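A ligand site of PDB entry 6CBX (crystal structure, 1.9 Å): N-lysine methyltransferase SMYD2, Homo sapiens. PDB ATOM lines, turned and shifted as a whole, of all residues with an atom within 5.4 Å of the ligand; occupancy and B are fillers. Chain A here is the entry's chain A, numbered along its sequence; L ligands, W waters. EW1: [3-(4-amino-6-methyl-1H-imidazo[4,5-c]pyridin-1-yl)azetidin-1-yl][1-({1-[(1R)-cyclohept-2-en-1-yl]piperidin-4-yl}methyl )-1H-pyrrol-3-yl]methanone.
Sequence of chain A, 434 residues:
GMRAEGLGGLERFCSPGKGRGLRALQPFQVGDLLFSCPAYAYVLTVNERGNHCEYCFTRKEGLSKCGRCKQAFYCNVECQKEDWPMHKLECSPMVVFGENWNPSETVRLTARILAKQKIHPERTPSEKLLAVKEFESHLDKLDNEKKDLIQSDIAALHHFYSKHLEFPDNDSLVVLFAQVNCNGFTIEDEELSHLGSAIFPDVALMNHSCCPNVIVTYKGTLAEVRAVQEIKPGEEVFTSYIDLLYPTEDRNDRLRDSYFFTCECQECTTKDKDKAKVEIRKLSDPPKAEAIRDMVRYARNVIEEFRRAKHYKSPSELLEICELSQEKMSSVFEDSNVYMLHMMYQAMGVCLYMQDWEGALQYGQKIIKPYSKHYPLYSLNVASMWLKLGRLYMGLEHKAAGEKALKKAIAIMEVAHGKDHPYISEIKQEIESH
The backbone NH (N) of His 208 sits at hydrogen-bond distance from a nitrogen (N) of the ligand, 2.9 Å away.
O of His 208 sits at hydrogen-bond distance from N5 of the ligand (3.0 Å).
O of the ligand sits at hydrogen-bond distance from NE2 of His 138, 2.7 Å away.
The side-chain carboxylate (OE1) of Glu 264 sits at hydrogen-bond distance from a nitrogen (N5) of the ligand.
The side-chain sulfur (SG) of Cys 182 sits at hydrogen-bond distance from the backbone carbonyl oxygen (O) of Glu 136 (3.2 Å).
N of Tyr 241 sits at hydrogen-bond distance from ND1 of His 208, 3.1 Å away.
The side-chain amide nitrogen (ND2) of Asn 183 sits at hydrogen-bond distance from the backbone carbonyl oxygen (O) of Glu 136, at 3.1 Å.
The side-chain amino group (NZ) of Lys 18 is in salt-bridge range of the side-chain carboxylate (OE1) of Glu 264, 3.6 Å away.
The backbone carbonyl oxygen (O) of Tyr 259 sits at hydrogen-bond distance from a ring nitrogen (NE2) of His 138 (3.3 Å).
The side-chain amide nitrogen of Asn 183 is in hydrogen-bond range of the side-chain sulfur of Cys 182 (3.5 Å).
O of Met 206 is in hydrogen-bond range of OH of Tyr 241 (2.6 Å).
OD1 of Asn 207 lies close to N1 of the ligand, 3.3 Å away.
O of the ligand sits close to O of Tyr 259 (3.3 Å).
Gly 17 touches the ligand.
Lys 18 touches the ligand.
Glu 136 touches the ligand (OE2 to N2, 3.6 Å).
O of Cys 182 touches C13 of the ligand, at 3.4 Å.
OD1 of Asn 183 touches C25 of the ligand (3.4 Å).
O of Gly 184 touches C23 of the ligand, at 3.2 Å.
Phe 185 touches the ligand.
O of Ala 204 touches C12 of the ligand (3.6 Å).
OH of Tyr 241 touches C5 of the ligand (3.3 Å).
Phe 261 touches the ligand (CE2 to C27, 3.3 Å).
Thr 262 touches the ligand (O to C, 3.9 Å).
Hydrophobic or aromatic side chains within 4 Å of the ligand: His 138, Phe 185, Ala 204, His 208, Tyr 241, Tyr 259 and Phe 261.
16 residues have an atom within 4 Å of the ligand: Gly 17, Lys 18, Glu 136, His 138, Cys 182, Asn 183, Gly 184, Phe 185, Ala 204, Asn 207, His 208, Tyr 241, Tyr 259, Phe 261, Thr 262 and Glu 264.
Along chain A the residues within 4 Å of the ligand span positions 17 to 264.
The nearest printed residue that does not touch the ligand is Thr 186 (4.2 Å).
Water W3 bridges O of Tyr 259 (2.7 Å) and O of the ligand (3.0 Å).
Water W2 lies within hydrogen-bond range of OD1 of Asn 207 and O of Lys 18.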
ATOM      1  N   GLY A  17     -11.789  24.820 -33.939  1.00  0.00           N
ATOM      2  CA  GLY A  17     -11.430  25.633 -32.813  1.00  0.00           C
ATOM      3  C   GLY A  17     -12.548  25.860 -31.802  1.00  0.00           C
ATOM      4  O   GLY A  17     -12.300  26.438 -30.741  1.00  0.00           O
ATOM      5  N   LYS A  18     -13.753  25.384 -32.127  1.00  0.00           N
ATOM      6  CA  LYS A  18     -14.957  25.658 -31.347  1.00  0.00           C
ATOM      7  C   LYS A  18     -15.647  24.420 -30.825  1.00  0.00           C
ATOM      8  O   LYS A  18     -16.105  24.427 -29.714  1.00  0.00           O
ATOM      9  CB  LYS A  18     -15.927  26.490 -32.187  1.00  0.00           C
ATOM     10  CG  LYS A  18     -15.371  27.819 -32.615  1.00  0.00           C
ATOM     11  CD  LYS A  18     -16.357  28.578 -33.477  1.00  0.00           C
ATOM     12  CE  LYS A  18     -15.912  29.992 -33.746  1.00  0.00           C
ATOM     13  NZ  LYS A  18     -14.685  30.059 -34.564  1.00  0.00           N
ATOM     14  N   GLU A 136     -22.600  19.893 -22.146  1.00  0.00           N
ATOM     15  CA  GLU A 136     -21.374  20.169 -21.419  1.00  0.00           C
ATOM     16  C   GLU A 136     -21.737  20.604 -19.985  1.00  0.00           C
ATOM     17  O   GLU A 136     -22.626  21.443 -19.801  1.00  0.00           O
ATOM     18  CB  GLU A 136     -20.569  21.245 -22.134  1.00  0.00           C
ATOM     19  CG  GLU A 136     -19.976  20.789 -23.464  1.00  0.00           C
ATOM     20  CD  GLU A 136     -18.949  21.741 -24.031  1.00  0.00           C
ATOM     21  OE1 GLU A 136     -17.867  21.887 -23.427  1.00  0.00           O
ATOM     22  OE2 GLU A 136     -19.210  22.351 -25.096  1.00  0.00           O
ATOM     23  N   HIS A 138     -18.986  21.284 -17.706  1.00  0.00           N
ATOM     24  CA  HIS A 138     -17.810  22.015 -17.239  1.00  0.00           C
ATOM     25  C   HIS A 138     -17.441  21.732 -15.784  1.00  0.00           C
ATOM     26  O   HIS A 138     -16.814  22.563 -15.135  1.00  0.00           O
ATOM     27  CB  HIS A 138     -17.964  23.536 -17.470  1.00  0.00           C
ATOM     28  CG  HIS A 138     -17.926  23.934 -18.913  1.00  0.00           C
ATOM     29  ND1 HIS A 138     -16.908  23.552 -19.750  1.00  0.00           N
ATOM     30  CD2 HIS A 138     -18.773  24.672 -19.655  1.00  0.00           C
ATOM     31  CE1 HIS A 138     -17.137  24.043 -20.964  1.00  0.00           C
ATOM     32  NE2 HIS A 138     -18.266  24.725 -20.928  1.00  0.00           N
ATOM     33  N   CYS A 182     -25.287  25.953 -17.265  1.00  0.00           N
ATOM     34  CA  CYS A 182     -24.761  26.607 -18.483  1.00  0.00           C
ATOM     35  C   CYS A 182     -25.618  26.415 -19.755  1.00  0.00           C
ATOM     36  O   CYS A 182     -25.443  27.161 -20.699  1.00  0.00           O
ATOM     37  CB  CYS A 182     -23.290  26.250 -18.706  1.00  0.00           C
ATOM     38  SG  CYS A 182     -22.940  24.539 -19.124  1.00  0.00           S
ATOM     39  N   ASN A 183     -26.550  25.473 -19.772  1.00  0.00           N
ATOM     40  CA  ASN A 183     -27.349  25.182 -20.974  1.00  0.00           C
ATOM     41  C   ASN A 183     -28.760  25.706 -20.942  1.00  0.00           C
ATOM     42  O   ASN A 183     -29.392  25.785 -21.989  1.00  0.00           O
ATOM     43  CB  ASN A 183     -27.384  23.677 -21.239  1.00  0.00           C
ATOM     44  CG  ASN A 183     -26.078  23.158 -21.722  1.00  0.00           C
ATOM     45  OD1 ASN A 183     -25.746  23.313 -22.895  1.00  0.00           O
ATOM     46  ND2 ASN A 183     -25.274  22.572 -20.825  1.00  0.00           N
ATOM     47  N   GLY A 184     -29.291  26.047 -19.756  1.00  0.00           N
ATOM     48  CA  GLY A 184     -30.637  26.607 -19.669  1.00  0.00           C
ATOM     49  C   GLY A 184     -30.783  27.930 -20.396  1.00  0.00           C
ATOM     50  O   GLY A 184     -29.864  28.761 -20.387  1.00  0.00           O
ATOM     51  N   PHE A 185     -31.936  28.119 -21.036  1.00  0.00           N
ATOM     52  CA  PHE A 185     -32.295  29.398 -21.673  1.00  0.00           C
ATOM     53  C   PHE A 185     -33.319  30.118 -20.819  1.00  0.00           C
ATOM     54  O   PHE A 185     -34.188  29.478 -20.245  1.00  0.00           O
ATOM     55  CB  PHE A 185     -32.908  29.152 -23.043  1.00  0.00           C
ATOM     56  CG  PHE A 185     -31.911  28.717 -24.073  1.00  0.00           C
ATOM     57  CD1 PHE A 185     -31.572  27.381 -24.206  1.00  0.00           C
ATOM     58  CD2 PHE A 185     -31.317  29.657 -24.913  1.00  0.00           C
ATOM     59  CE1 PHE A 185     -30.661  26.974 -25.177  1.00  0.00           C
ATOM     60  CE2 PHE A 185     -30.399  29.261 -25.883  1.00  0.00           C
ATOM     61  CZ  PHE A 185     -30.073  27.917 -26.009  1.00  0.00           C
ATOM     62  N   THR A 186     -33.257  31.446 -20.773  1.00  0.00           N
ATOM     63  CA  THR A 186     -34.307  32.239 -20.145  1.00  0.00           C
ATOM     64  C   THR A 186     -35.281  32.644 -21.238  1.00  0.00           C
ATOM     65  O   THR A 186     -34.890  33.081 -22.296  1.00  0.00           O
ATOM     66  CB  THR A 186     -33.726  33.463 -19.411  1.00  0.00           C
ATOM     67  OG1 THR A 186     -32.813  34.145 -20.280  1.00  0.00           O
ATOM     68  CG2 THR A 186     -32.948  33.039 -18.228  1.00  0.00           C
ATOM     69  N   ALA A 204     -29.027  24.721 -28.145  1.00  0.00           N
ATOM     70  CA  ALA A 204     -27.733  24.677 -27.427  1.00  0.00           C
ATOM     71  C   ALA A 204     -26.535  24.200 -28.290  1.00  0.00           C
ATOM     72  O   ALA A 204     -25.377  24.321 -27.875  1.00  0.00           O
ATOM     73  CB  ALA A 204     -27.859  23.840 -26.164  1.00  0.00           C
ATOM     74  N   MET A 206     -25.671  25.451 -31.210  1.00  0.00           N
ATOM     75  CA  MET A 206     -25.070  26.568 -31.895  1.00  0.00           C
ATOM     76  C   MET A 206     -23.887  27.179 -31.125  1.00  0.00           C
ATOM     77  O   MET A 206     -23.924  27.342 -29.896  1.00  0.00           O
ATOM     78  CB  MET A 206     -26.105  27.627 -32.237  1.00  0.00           C
ATOM     79  CG  MET A 206     -27.165  27.141 -33.206  1.00  0.00           C
ATOM     80  SD  MET A 206     -28.309  28.481 -33.637  1.00  0.00           S
ATOM     81  CE  MET A 206     -29.185  28.740 -32.101  1.00  0.00           C
ATOM     82  N   ASN A 207     -22.827  27.473 -31.880  1.00  0.00           N
ATOM     83  CA  ASN A 207     -21.679  28.155 -31.316  1.00  0.00           C
ATOM     84  C   ASN A 207     -21.925  29.656 -31.241  1.00  0.00           C
ATOM     85  O   ASN A 207     -22.909  30.175 -31.774  1.00  0.00           O
ATOM     86  CB  ASN A 207     -20.388  27.803 -32.088  1.00  0.00           C
ATOM     87  CG  ASN A 207     -19.856  26.408 -31.732  1.00  0.00           C
ATOM     88  OD1 ASN A 207     -19.856  26.001 -30.570  1.00  0.00           O
ATOM     89  ND2 ASN A 207     -19.424  25.678 -32.739  1.00  0.00           N
ATOM     90  N   HIS A 208     -21.027  30.322 -30.535  1.00  0.00           N
ATOM     91  CA  HIS A 208     -21.094  31.730 -30.228  1.00  0.00           C
ATOM     92  C   HIS A 208     -20.256  32.566 -31.185  1.00  0.00           C
ATOM     93  O   HIS A 208     -19.126  32.178 -31.517  1.00  0.00           O
ATOM     94  CB  HIS A 208     -20.603  32.011 -28.801  1.00  0.00           C
ATOM     95  CG  HIS A 208     -20.328  33.458 -28.560  1.00  0.00           C
ATOM     96  ND1 HIS A 208     -21.320  34.333 -28.206  1.00  0.00           N
ATOM     97  CD2 HIS A 208     -19.219  34.207 -28.772  1.00  0.00           C
ATOM     98  CE1 HIS A 208     -20.824  35.560 -28.132  1.00  0.00           C
ATOM     99  NE2 HIS A 208     -19.554  35.510 -28.501  1.00  0.00           N
ATOM    100  N   SER A 209     -20.796  33.714 -31.598  1.00  0.00           N
ATOM    101  CA  SER A 209     -20.053  34.834 -32.157  1.00  0.00           C
ATOM    102  C   SER A 209     -20.625  36.161 -31.615  1.00  0.00           C
ATOM    103  O   SER A 209     -21.820  36.259 -31.300  1.00  0.00           O
ATOM    104  CB  SER A 209     -20.119  34.824 -33.701  1.00  0.00           C
ATOM    105  OG  SER A 209     -19.522  35.966 -34.262  1.00  0.00           O
ATOM    106  N   SER A 240     -25.465  34.471 -30.247  1.00  0.00           N
ATOM    107  CA  SER A 240     -24.681  35.086 -29.177  1.00  0.00           C
ATOM    108  C   SER A 240     -25.108  34.548 -27.811  1.00  0.00           C
ATOM    109  O   SER A 240     -26.289  34.451 -27.533  1.00  0.00           O
ATOM    110  CB  SER A 240     -24.788  36.627 -29.162  1.00  0.00           C
ATOM    111  OG  SER A 240     -24.065  37.112 -28.026  1.00  0.00           O
ATOM    112  N   TYR A 241     -24.141  34.242 -26.967  1.00  0.00           N
ATOM    113  CA  TYR A 241     -24.389  33.740 -25.647  1.00  0.00           C
ATOM    114  C   TYR A 241     -24.410  34.895 -24.657  1.00  0.00           C
ATOM    115  O   TYR A 241     -24.847  34.688 -23.521  1.00  0.00           O
ATOM    116  CB  TYR A 241     -23.264  32.803 -25.166  1.00  0.00           C
ATOM    117  CG  TYR A 241     -23.034  31.517 -25.916  1.00  0.00           C
ATOM    118  CD1 TYR A 241     -23.849  31.102 -26.962  1.00  0.00           C
ATOM    119  CD2 TYR A 241     -21.969  30.674 -25.543  1.00  0.00           C
ATOM    120  CE1 TYR A 241     -23.595  29.912 -27.631  1.00  0.00           C
ATOM    121  CE2 TYR A 241     -21.720  29.487 -26.204  1.00  0.00           C
ATOM    122  CZ  TYR A 241     -22.534  29.115 -27.251  1.00  0.00           C
ATOM    123  OH  TYR A 241     -22.296  27.923 -27.892  1.00  0.00           O
ATOM    124  N   ILE A 242     -23.919  36.078 -25.065  1.00  0.00           N
ATOM    125  CA  ILE A 242     -23.714  37.186 -24.125  1.00  0.00           C
ATOM    126  C   ILE A 242     -24.358  38.468 -24.649  1.00  0.00           C
ATOM    127  O   ILE A 242     -24.834  38.526 -25.776  1.00  0.00           O
ATOM    128  CB  ILE A 242     -22.221  37.389 -23.721  1.00  0.00           C
ATOM    129  CG1 ILE A 242     -21.237  37.392 -24.920  1.00  0.00           C
ATOM    130  CG2 ILE A 242     -21.790  36.310 -22.735  1.00  0.00           C
ATOM    131  CD1 ILE A 242     -21.239  38.668 -25.736  1.00  0.00           C
ATOM    132  N   TYR A 259     -18.797  29.872 -19.494  1.00  0.00           N
ATOM    133  CA  TYR A 259     -18.515  28.813 -20.473  1.00  0.00           C
ATOM    134  C   TYR A 259     -17.023  28.486 -20.619  1.00  0.00           C
ATOM    135  O   TYR A 259     -16.690  27.574 -21.356  1.00  0.00           O
ATOM    136  CB  TYR A 259     -19.093  29.179 -21.843  1.00  0.00           C
ATOM    137  CG  TYR A 259     -20.487  29.741 -21.714  1.00  0.00           C
ATOM    138  CD1 TYR A 259     -21.560  28.913 -21.378  1.00  0.00           C
ATOM    139  CD2 TYR A 259     -20.720  31.107 -21.831  1.00  0.00           C
ATOM    140  CE1 TYR A 259     -22.832  29.438 -21.196  1.00  0.00           C
ATOM    141  CE2 TYR A 259     -21.984  31.644 -21.648  1.00  0.00           C
ATOM    142  CZ  TYR A 259     -23.037  30.813 -21.349  1.00  0.00           C
ATOM    143  OH  TYR A 259     -24.297  31.366 -21.181  1.00  0.00           O
ATOM    144  N   PHE A 261     -14.477  29.778 -22.095  1.00  0.00           N
ATOM    145  CA  PHE A 261     -13.787  29.996 -23.357  1.00  0.00           C
ATOM    146  C   PHE A 261     -13.789  31.472 -23.673  1.00  0.00           C
ATOM    147  O   PHE A 261     -14.529  32.248 -23.088  1.00  0.00           O
ATOM    148  CB  PHE A 261     -14.423  29.187 -24.514  1.00  0.00           C
ATOM    149  CG  PHE A 261     -15.726  29.752 -25.044  1.00  0.00           C
ATOM    150  CD1 PHE A 261     -16.942  29.360 -24.491  1.00  0.00           C
ATOM    151  CD2 PHE A 261     -15.738  30.664 -26.113  1.00  0.00           C
ATOM    152  CE1 PHE A 261     -18.158  29.838 -25.010  1.00  0.00           C
ATOM    153  CE2 PHE A 261     -16.947  31.161 -26.610  1.00  0.00           C
ATOM    154  CZ  PHE A 261     -18.143  30.739 -26.058  1.00  0.00           C
ATOM    155  N   THR A 262     -12.914  31.851 -24.601  1.00  0.00           N
ATOM    156  CA  THR A 262     -12.812  33.222 -25.098  1.00  0.00           C
ATOM    157  C   THR A 262     -13.133  33.217 -26.585  1.00  0.00           C
ATOM    158  O   THR A 262     -12.873  32.240 -27.285  1.00  0.00           O
ATOM    159  CB  THR A 262     -11.407  33.794 -24.864  1.00  0.00           C
ATOM    160  OG1 THR A 262     -10.449  32.929 -25.440  1.00  0.00           O
ATOM    161  CG2 THR A 262     -11.104  33.905 -23.375  1.00  0.00           C
ATOM    162  N   CYS A 263     -13.693  34.327 -27.071  1.00  0.00           N
ATOM    163  CA  CYS A 263     -14.186  34.420 -28.442  1.00  0.00           C
ATOM    164  C   CYS A 263     -13.069  34.824 -29.396  1.00  0.00           C
ATOM    165  O   CYS A 263     -12.165  35.536 -29.023  1.00  0.00           O
ATOM    166  CB  CYS A 263     -15.324  35.423 -28.547  1.00  0.00           C
ATOM    167  SG  CYS A 263     -16.126  35.410 -30.177  1.00  0.00           S
ATOM    168  N   GLU A 264     -13.192  34.386 -30.647  1.00  0.00           N
ATOM    169  CA  GLU A 264     -12.225  34.654 -31.711  1.00  0.00           C
ATOM    170  C   GLU A 264     -12.858  35.310 -32.931  1.00  0.00           C
ATOM    171  O   GLU A 264     -12.193  35.454 -33.961  1.00  0.00           O
ATOM    172  CB  GLU A 264     -11.478  33.359 -32.116  1.00  0.00           C
ATOM    173  CG  GLU A 264     -12.345  32.209 -32.663  1.00  0.00           C
ATOM    174  CD  GLU A 264     -13.355  31.665 -31.643  1.00  0.00           C
ATOM    175  OE1 GLU A 264     -14.513  32.130 -31.639  1.00  0.00           O
ATOM    176  OE2 GLU A 264     -12.985  30.855 -30.787  1.00  0.00           O
HETATM  177  C4  EW1 L   1     -17.357  29.063 -29.172  1.00  0.00           C
HETATM  178  C5  EW1 L   1     -19.129  28.024 -28.656  1.00  0.00           C
HETATM  179  C6  EW1 L   1     -18.208  26.009 -27.422  1.00  0.00           C
HETATM  180  N1  EW1 L   1     -18.111  27.277 -28.135  1.00  0.00           N
HETATM  181  C7  EW1 L   1     -19.628  25.658 -26.902  1.00  0.00           C
HETATM  182  C8  EW1 L   1     -17.749  26.163 -25.959  1.00  0.00           C
HETATM  183  N2  EW1 L   1     -19.124  25.875 -25.531  1.00  0.00           N
HETATM  184  C9  EW1 L   1     -19.530  25.839 -24.260  1.00  0.00           C
HETATM  185  C10 EW1 L   1     -20.970  25.680 -23.990  1.00  0.00           C
HETATM  186  C11 EW1 L   1     -22.004  25.948 -24.865  1.00  0.00           C
HETATM  187  C12 EW1 L   1     -24.516  25.917 -24.818  1.00  0.00           C
HETATM  188  N3  EW1 L   1     -23.193  25.679 -24.250  1.00  0.00           N
HETATM  189  C13 EW1 L   1     -25.271  26.990 -24.096  1.00  0.00           C
HETATM  190  C14 EW1 L   1     -24.664  28.353 -24.356  1.00  0.00           C
HETATM  191  C15 EW1 L   1     -25.403  29.438 -23.604  1.00  0.00           C
HETATM  192  N4  EW1 L   1     -26.851  29.447 -23.938  1.00  0.00           N
HETATM  193  O   EW1 L   1     -18.724  25.799 -23.337  1.00  0.00           O
HETATM  194  C3  EW1 L   1     -16.950  27.949 -28.448  1.00  0.00           C
HETATM  195  C2  EW1 L   1     -15.612  27.656 -28.222  1.00  0.00           C
HETATM  196  N   EW1 L   1     -18.734  29.105 -29.288  1.00  0.00           N
HETATM  197  C27 EW1 L   1     -16.369  29.929 -29.648  1.00  0.00           C
HETATM  198  N5  EW1 L   1     -16.649  31.015 -30.356  1.00  0.00           N
HETATM  199  N6  EW1 L   1     -15.064  29.682 -29.385  1.00  0.00           N
HETATM  200  C1  EW1 L   1     -14.692  28.608 -28.660  1.00  0.00           C
HETATM  201  C   EW1 L   1     -13.229  28.510 -28.310  1.00  0.00           C
HETATM  202  C26 EW1 L   1     -21.575  25.217 -22.764  1.00  0.00           C
HETATM  203  C25 EW1 L   1     -22.918  25.236 -22.974  1.00  0.00           C
HETATM  204  C17 EW1 L   1     -26.743  27.043 -24.450  1.00  0.00           C
HETATM  205  C16 EW1 L   1     -27.444  28.123 -23.659  1.00  0.00           C
HETATM  206  C18 EW1 L   1     -27.629  30.614 -23.498  1.00  0.00           C
HETATM  207  C24 EW1 L   1     -27.624  30.636 -21.998  1.00  0.00           C
HETATM  208  C23 EW1 L   1     -28.313  31.478 -21.217  1.00  0.00           C
HETATM  209  C22 EW1 L   1     -29.186  32.600 -21.674  1.00  0.00           C
HETATM  210  C21 EW1 L   1     -28.473  33.642 -22.546  1.00  0.00           C
HETATM  211  C20 EW1 L   1     -28.250  33.085 -23.942  1.00  0.00           C
HETATM  212  C19 EW1 L   1     -27.199  31.982 -24.057  1.00  0.00           C
HETATM  213  O   HOH W   1     -27.002  29.820 -26.777  1.00  0.00           O
HETATM  214  O   HOH W   2     -19.420  23.460 -29.431  1.00  0.00           O
HETATM  215  O   HOH W   3     -15.723  25.840 -23.211  1.00  0.00           O
